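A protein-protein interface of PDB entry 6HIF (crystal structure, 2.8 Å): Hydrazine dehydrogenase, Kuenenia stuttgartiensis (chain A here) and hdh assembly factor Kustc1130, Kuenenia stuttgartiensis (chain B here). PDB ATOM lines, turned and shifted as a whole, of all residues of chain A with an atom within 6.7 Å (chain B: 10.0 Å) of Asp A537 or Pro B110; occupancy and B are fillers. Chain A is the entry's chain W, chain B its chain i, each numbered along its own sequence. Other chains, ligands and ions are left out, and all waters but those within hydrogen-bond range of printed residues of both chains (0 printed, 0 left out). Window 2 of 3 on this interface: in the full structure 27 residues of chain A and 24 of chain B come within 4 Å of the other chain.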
ATOM      1  N   LYS A  81      15.184 -12.972 -24.284  1.00  0.00           N
ATOM      2  CA  LYS A  81      14.061 -12.152 -23.859  1.00  0.00           C
ATOM      3  C   LYS A  81      14.088 -10.793 -24.554  1.00  0.00           C
ATOM      4  O   LYS A  81      13.042 -10.290 -24.956  1.00  0.00           O
ATOM      5  CB  LYS A  81      14.139 -11.980 -22.337  1.00  0.00           C
ATOM      6  CG  LYS A  81      12.901 -11.428 -21.641  1.00  0.00           C
ATOM      7  CD  LYS A  81      13.164 -11.125 -20.175  1.00  0.00           C
ATOM      8  CE  LYS A  81      11.921 -11.094 -19.309  1.00  0.00           C
ATOM      9  NZ  LYS A  81      11.016  -9.978 -19.670  1.00  0.00           N
ATOM     10  N   PRO A 531       7.938  -9.106 -23.182  1.00  0.00           N
ATOM     11  CA  PRO A 531       7.147  -9.841 -22.194  1.00  0.00           C
ATOM     12  C   PRO A 531       7.530 -11.311 -22.040  1.00  0.00           C
ATOM     13  O   PRO A 531       7.068 -11.973 -21.113  1.00  0.00           O
ATOM     14  CB  PRO A 531       5.723  -9.717 -22.757  1.00  0.00           C
ATOM     15  CG  PRO A 531       5.917  -9.681 -24.260  1.00  0.00           C
ATOM     16  CD  PRO A 531       7.243  -8.977 -24.475  1.00  0.00           C
ATOM     17  N   ASP A 532       8.378 -11.806 -22.951  1.00  0.00           N
ATOM     18  CA  ASP A 532       8.771 -13.207 -22.993  1.00  0.00           C
ATOM     19  C   ASP A 532       9.412 -13.616 -21.667  1.00  0.00           C
ATOM     20  O   ASP A 532       9.983 -12.778 -20.972  1.00  0.00           O
ATOM     21  CB  ASP A 532       9.705 -13.481 -24.174  1.00  0.00           C
ATOM     22  CG  ASP A 532       9.025 -13.392 -25.531  1.00  0.00           C
ATOM     23  OD1 ASP A 532       7.780 -13.468 -25.575  1.00  0.00           O
ATOM     24  OD2 ASP A 532       9.746 -13.255 -26.535  1.00  0.00           O
ATOM     25  N   PRO A 533       9.320 -14.908 -21.265  1.00  0.00           N
ATOM     26  CA  PRO A 533       9.975 -15.383 -20.045  1.00  0.00           C
ATOM     27  C   PRO A 533      11.495 -15.299 -20.166  1.00  0.00           C
ATOM     28  O   PRO A 533      12.055 -15.609 -21.217  1.00  0.00           O
ATOM     29  CB  PRO A 533       9.549 -16.856 -19.933  1.00  0.00           C
ATOM     30  CG  PRO A 533       8.332 -16.973 -20.827  1.00  0.00           C
ATOM     31  CD  PRO A 533       8.562 -15.973 -21.941  1.00  0.00           C
ATOM     32  N   GLY A 534      12.141 -14.867 -19.077  1.00  0.00           N
ATOM     33  CA  GLY A 534      13.589 -14.744 -19.014  1.00  0.00           C
ATOM     34  C   GLY A 534      14.254 -16.039 -18.556  1.00  0.00           C
ATOM     35  O   GLY A 534      13.596 -17.069 -18.414  1.00  0.00           O
ATOM     36  N   TRP A 535      15.569 -15.963 -18.323  1.00  0.00           N
ATOM     37  CA  TRP A 535      16.366 -17.116 -17.937  1.00  0.00           C
ATOM     38  C   TRP A 535      15.955 -17.592 -16.548  1.00  0.00           C
ATOM     39  O   TRP A 535      15.871 -18.794 -16.309  1.00  0.00           O
ATOM     40  CB  TRP A 535      17.862 -16.786 -18.003  1.00  0.00           C
ATOM     41  CG  TRP A 535      18.757 -17.964 -17.757  1.00  0.00           C
ATOM     42  CD1 TRP A 535      19.254 -18.828 -18.690  1.00  0.00           C
ATOM     43  CD2 TRP A 535      19.264 -18.413 -16.487  1.00  0.00           C
ATOM     44  NE1 TRP A 535      20.034 -19.780 -18.091  1.00  0.00           N
ATOM     45  CE2 TRP A 535      20.060 -19.552 -16.739  1.00  0.00           C
ATOM     46  CE3 TRP A 535      19.130 -17.969 -15.167  1.00  0.00           C
ATOM     47  CZ2 TRP A 535      20.711 -20.247 -15.719  1.00  0.00           C
ATOM     48  CZ3 TRP A 535      19.774 -18.654 -14.159  1.00  0.00           C
ATOM     49  CH2 TRP A 535      20.555 -19.778 -14.434  1.00  0.00           C
ATOM     50  N   LEU A 536      15.690 -16.632 -15.652  1.00  0.00           N
ATOM     51  CA  LEU A 536      15.381 -16.910 -14.258  1.00  0.00           C
ATOM     52  C   LEU A 536      14.024 -17.603 -14.136  1.00  0.00           C
ATOM     53  O   LEU A 536      13.761 -18.274 -13.140  1.00  0.00           O
ATOM     54  CB  LEU A 536      15.404 -15.599 -13.463  1.00  0.00           C
ATOM     55  CG  LEU A 536      16.790 -15.041 -13.141  1.00  0.00           C
ATOM     56  CD1 LEU A 536      16.711 -13.572 -12.755  1.00  0.00           C
ATOM     57  CD2 LEU A 536      17.466 -15.850 -12.041  1.00  0.00           C
ATOM     58  N   ASP A 537      13.180 -17.439 -15.161  1.00  0.00           N
ATOM     59  CA  ASP A 537      11.833 -17.988 -15.161  1.00  0.00           C
ATOM     60  C   ASP A 537      11.875 -19.490 -15.431  1.00  0.00           C
ATOM     61  O   ASP A 537      10.984 -20.216 -14.995  1.00  0.00           O
ATOM     62  CB  ASP A 537      10.929 -17.258 -16.159  1.00  0.00           C
ATOM     63  CG  ASP A 537      10.713 -15.789 -15.828  1.00  0.00           C
ATOM     64  OD1 ASP A 537      10.567 -15.472 -14.632  1.00  0.00           O
ATOM     65  OD2 ASP A 537      10.696 -14.971 -16.770  1.00  0.00           O
ATOM     66  N   THR A 538      12.921 -19.941 -16.138  1.00  0.00           N
ATOM     67  CA  THR A 538      12.999 -21.308 -16.633  1.00  0.00           C
ATOM     68  C   THR A 538      14.125 -22.086 -15.949  1.00  0.00           C
ATOM     69  O   THR A 538      14.214 -23.302 -16.102  1.00  0.00           O
ATOM     70  CB  THR A 538      13.124 -21.332 -18.162  1.00  0.00           C
ATOM     71  OG1 THR A 538      14.217 -20.490 -18.530  1.00  0.00           O
ATOM     72  CG2 THR A 538      11.874 -20.853 -18.868  1.00  0.00           C
ATOM     73  N   HIS A 539      14.977 -21.380 -15.195  1.00  0.00           N
ATOM     74  CA  HIS A 539      16.121 -21.995 -14.541  1.00  0.00           C
ATOM     75  C   HIS A 539      16.084 -21.719 -13.039  1.00  0.00           C
ATOM     76  O   HIS A 539      16.036 -20.565 -12.617  1.00  0.00           O
ATOM     77  CB  HIS A 539      17.430 -21.520 -15.185  1.00  0.00           C
ATOM     78  CG  HIS A 539      17.548 -21.851 -16.637  1.00  0.00           C
ATOM     79  ND1 HIS A 539      18.204 -22.979 -17.089  1.00  0.00           N
ATOM     80  CD2 HIS A 539      17.104 -21.208 -17.738  1.00  0.00           C
ATOM     81  CE1 HIS A 539      18.160 -23.017 -18.406  1.00  0.00           C
ATOM     82  NE2 HIS A 539      17.490 -21.940 -18.829  1.00  0.00           N
ATOM     83  N   HIS A 540      16.119 -22.798 -12.247  1.00  0.00           N
ATOM     84  CA  HIS A 540      16.002 -22.720 -10.800  1.00  0.00           C
ATOM     85  C   HIS A 540      17.197 -23.412 -10.149  1.00  0.00           C
ATOM     86  O   HIS A 540      17.936 -24.134 -10.816  1.00  0.00           O
ATOM     87  CB  HIS A 540      14.665 -23.325 -10.341  1.00  0.00           C
ATOM     88  CG  HIS A 540      13.493 -22.905 -11.166  1.00  0.00           C
ATOM     89  ND1 HIS A 540      12.886 -21.668 -11.021  1.00  0.00           N
ATOM     90  CD2 HIS A 540      12.816 -23.545 -12.144  1.00  0.00           C
ATOM     91  CE1 HIS A 540      11.885 -21.567 -11.873  1.00  0.00           C
ATOM     92  NE2 HIS A 540      11.820 -22.706 -12.574  1.00  0.00           N
ATOM     93  N   ALA B  39      14.821 -22.650 -28.717  1.00  0.00           N
ATOM     94  CA  ALA B  39      13.768 -21.706 -28.385  1.00  0.00           C
ATOM     95  C   ALA B  39      14.404 -20.354 -28.065  1.00  0.00           C
ATOM     96  O   ALA B  39      14.822 -20.116 -26.932  1.00  0.00           O
ATOM     97  CB  ALA B  39      12.947 -22.229 -27.231  1.00  0.00           C
ATOM     98  N   THR B  42      18.005 -20.859 -26.483  1.00  0.00           N
ATOM     99  CA  THR B  42      18.159 -21.926 -25.507  1.00  0.00           C
ATOM    100  C   THR B  42      17.715 -23.256 -26.113  1.00  0.00           C
ATOM    101  O   THR B  42      16.746 -23.303 -26.871  1.00  0.00           O
ATOM    102  CB  THR B  42      17.446 -21.589 -24.189  1.00  0.00           C
ATOM    103  OG1 THR B  42      16.137 -21.099 -24.485  1.00  0.00           O
ATOM    104  CG2 THR B  42      18.197 -20.572 -23.354  1.00  0.00           C
ATOM    105  N   VAL B  45      14.574 -29.151 -24.335  1.00  0.00           N
ATOM    106  CA  VAL B  45      14.757 -30.469 -23.744  1.00  0.00           C
ATOM    107  C   VAL B  45      13.435 -31.231 -23.817  1.00  0.00           C
ATOM    108  O   VAL B  45      12.391 -30.717 -23.416  1.00  0.00           O
ATOM    109  CB  VAL B  45      15.281 -30.373 -22.295  1.00  0.00           C
ATOM    110  CG1 VAL B  45      15.486 -31.744 -21.666  1.00  0.00           C
ATOM    111  CG2 VAL B  45      16.556 -29.547 -22.199  1.00  0.00           C
ATOM    112  N   GLU B  79       7.170 -30.256 -29.817  1.00  0.00           N
ATOM    113  CA  GLU B  79       7.384 -30.114 -28.385  1.00  0.00           C
ATOM    114  C   GLU B  79       6.036 -29.904 -27.695  1.00  0.00           C
ATOM    115  O   GLU B  79       5.121 -29.325 -28.280  1.00  0.00           O
ATOM    116  CB  GLU B  79       8.467 -29.064 -28.111  1.00  0.00           C
ATOM    117  CG  GLU B  79       8.182 -28.128 -26.948  1.00  0.00           C
ATOM    118  CD  GLU B  79       7.456 -26.851 -27.334  1.00  0.00           C
ATOM    119  OE1 GLU B  79       7.518 -26.466 -28.518  1.00  0.00           O
ATOM    120  OE2 GLU B  79       6.829 -26.244 -26.450  1.00  0.00           O
ATOM    121  N   GLY B  81       4.523 -28.131 -25.828  1.00  0.00           N
ATOM    122  CA  GLY B  81       3.855 -26.841 -25.740  1.00  0.00           C
ATOM    123  C   GLY B  81       2.852 -26.629 -26.873  1.00  0.00           C
ATOM    124  O   GLY B  81       1.875 -25.900 -26.711  1.00  0.00           O
ATOM    125  N   ALA B 105       9.676 -18.195 -28.961  1.00  0.00           N
ATOM    126  CA  ALA B 105       9.704 -17.949 -27.527  1.00  0.00           C
ATOM    127  C   ALA B 105       8.632 -18.766 -26.807  1.00  0.00           C
ATOM    128  O   ALA B 105       8.730 -18.982 -25.600  1.00  0.00           O
ATOM    129  CB  ALA B 105       9.540 -16.472 -27.265  1.00  0.00           C
ATOM    130  N   LYS B 106       7.619 -19.213 -27.559  1.00  0.00           N
ATOM    131  CA  LYS B 106       6.500 -19.964 -27.010  1.00  0.00           C
ATOM    132  C   LYS B 106       6.939 -21.386 -26.661  1.00  0.00           C
ATOM    133  O   LYS B 106       6.221 -22.103 -25.966  1.00  0.00           O
ATOM    134  CB  LYS B 106       5.328 -19.979 -27.999  1.00  0.00           C
ATOM    135  CG  LYS B 106       4.590 -18.657 -28.173  1.00  0.00           C
ATOM    136  CD  LYS B 106       3.655 -18.653 -29.366  1.00  0.00           C
ATOM    137  CE  LYS B 106       3.013 -17.310 -29.638  1.00  0.00           C
ATOM    138  NZ  LYS B 106       1.921 -17.019 -28.678  1.00  0.00           N
ATOM    139  N   ALA B 107       8.126 -21.777 -27.142  1.00  0.00           N
ATOM    140  CA  ALA B 107       8.654 -23.120 -26.956  1.00  0.00           C
ATOM    141  C   ALA B 107       9.525 -23.190 -25.702  1.00  0.00           C
ATOM    142  O   ALA B 107      10.106 -24.233 -25.405  1.00  0.00           O
ATOM    143  CB  ALA B 107       9.423 -23.542 -28.183  1.00  0.00           C
ATOM    144  N   ARG B 108       9.599 -22.069 -24.972  1.00  0.00           N
ATOM    145  CA  ARG B 108      10.412 -21.951 -23.773  1.00  0.00           C
ATOM    146  C   ARG B 108       9.521 -22.154 -22.548  1.00  0.00           C
ATOM    147  O   ARG B 108       8.601 -21.372 -22.313  1.00  0.00           O
ATOM    148  CB  ARG B 108      11.094 -20.579 -23.755  1.00  0.00           C
ATOM    149  CG  ARG B 108      12.419 -20.534 -23.009  1.00  0.00           C
ATOM    150  CD  ARG B 108      13.037 -19.153 -23.126  1.00  0.00           C
ATOM    151  NE  ARG B 108      14.341 -19.049 -22.485  1.00  0.00           N
ATOM    152  CZ  ARG B 108      15.084 -17.947 -22.447  1.00  0.00           C
ATOM    153  NH1 ARG B 108      14.647 -16.827 -22.997  1.00  0.00           N
ATOM    154  NH2 ARG B 108      16.267 -17.972 -21.858  1.00  0.00           N
ATOM    155  N   HIS B 109       9.809 -23.209 -21.775  1.00  0.00           N
ATOM    156  CA  HIS B 109       8.958 -23.622 -20.668  1.00  0.00           C
ATOM    157  C   HIS B 109       9.737 -23.618 -19.354  1.00  0.00           C
ATOM    158  O   HIS B 109      10.890 -24.046 -19.318  1.00  0.00           O
ATOM    159  CB  HIS B 109       8.328 -24.992 -20.959  1.00  0.00           C
ATOM    160  CG  HIS B 109       7.370 -24.978 -22.101  1.00  0.00           C
ATOM    161  ND1 HIS B 109       6.174 -24.287 -22.051  1.00  0.00           N
ATOM    162  CD2 HIS B 109       7.421 -25.562 -23.317  1.00  0.00           C
ATOM    163  CE1 HIS B 109       5.532 -24.444 -23.190  1.00  0.00           C
ATOM    164  NE2 HIS B 109       6.276 -25.223 -23.982  1.00  0.00           N
ATOM    165  N   PRO B 110       9.129 -23.134 -18.240  1.00  0.00           N
ATOM    166  CA  PRO B 110       9.779 -23.137 -16.924  1.00  0.00           C
ATOM    167  C   PRO B 110      10.293 -24.507 -16.483  1.00  0.00           C
ATOM    168  O   PRO B 110       9.610 -25.515 -16.659  1.00  0.00           O
ATOM    169  CB  PRO B 110       8.673 -22.648 -15.976  1.00  0.00           C
ATOM    170  CG  PRO B 110       7.776 -21.810 -16.860  1.00  0.00           C
ATOM    171  CD  PRO B 110       7.791 -22.520 -18.197  1.00  0.00           C
ATOM    172  N   SER B 111      11.504 -24.510 -15.905  1.00  0.00           N
ATOM    173  CA  SER B 111      12.220 -25.701 -15.461  1.00  0.00           C
ATOM    174  C   SER B 111      12.304 -26.738 -16.590  1.00  0.00           C
ATOM    175  O   SER B 111      13.245 -27.530 -16.653  1.00  0.00           O
ATOM    176  CB  SER B 111      11.635 -26.281 -14.193  1.00  0.00           C
ATOM    177  OG  SER B 111      10.452 -27.020 -14.460  1.00  0.00           O
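O of Pro A533 sits at hydrogen-bond distance from NH1 of Arg B108 (3.4 Å). O of Thr A538 is in hydrogen-bond range of N of Ser B111.
The guanidinium group of Arg B108 is in hydrogen-bond range of the side-chain hydroxyl of Thr B42, 3.4 Å away. The backbone carbonyl oxygen (O) of Gly A534 sits at hydrogen-bond distance from the side-chain hydroxyl (OG1) of Thr A538 (3.5 Å). OE2 of Glu B79 lies within hydrogen-bond range of NE2 of His B109 (2.7 Å). The backbone carbonyl oxygen (O) of Trp A535 is in hydrogen-bond range of the side-chain hydroxyl (OG1) of Thr A538, 3.2 Å away. The backbone NH (N) of Gly A534 is in hydrogen-bond range of the side-chain carboxylate (OD2) of Asp A537 (2.7 Å). The side-chain amino group of Lys A81 sits close to the backbone carbonyl oxygen of Asp A532 (3.3 Å).
Asp A532 touches Ala B105 (OD2 to CB, 3.3 Å). Asp A537 touches Pro B110 (O to CB, 3.5 Å). His B109 touches Thr A538. CG2 of Thr A538 touches N of Pro B110, 3.6 Å away. Ser B111 touches His A540 (CB to CD2, 3.6 Å).
Printed residues of chain B within 4 Å of Asp A532: Ala B105. Pro A533 touches just one residue of chain B: Arg B108 (3.4 Å). Trp A535 touches none of the printed residues of chain B. Asp A537 touches just one residue of chain B: Pro B110 (3.5 Å). His A539 touches none of the printed residues of chain B. Of the printed residues of chain B, His A540 touches Ser B111. Printed residues of chain A within 4 Å of Ala B105: Asp A532 (3.3 Å). Of the printed residues of chain A, His B109 touches Thr A538 (3.4 Å). Pro B110 touches two residues of chain A. The nearest residue of chain B that does not touch Asp A537 is Ser B111 (4.4 Å).
Hydrophobic or aromatic side chains of chain B that line the printed part of chain A: Ala B105 and Pro B110. Along chain B the printed residues that touch a printed residue of chain A span positions 105 to 111. Among the printed residues, 7 pairs touch across the chains. Among the printed residues, no Asp or Glu carboxylate lies within 4 Å of a Lys or Arg side-chain nitrogen of the other chain.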
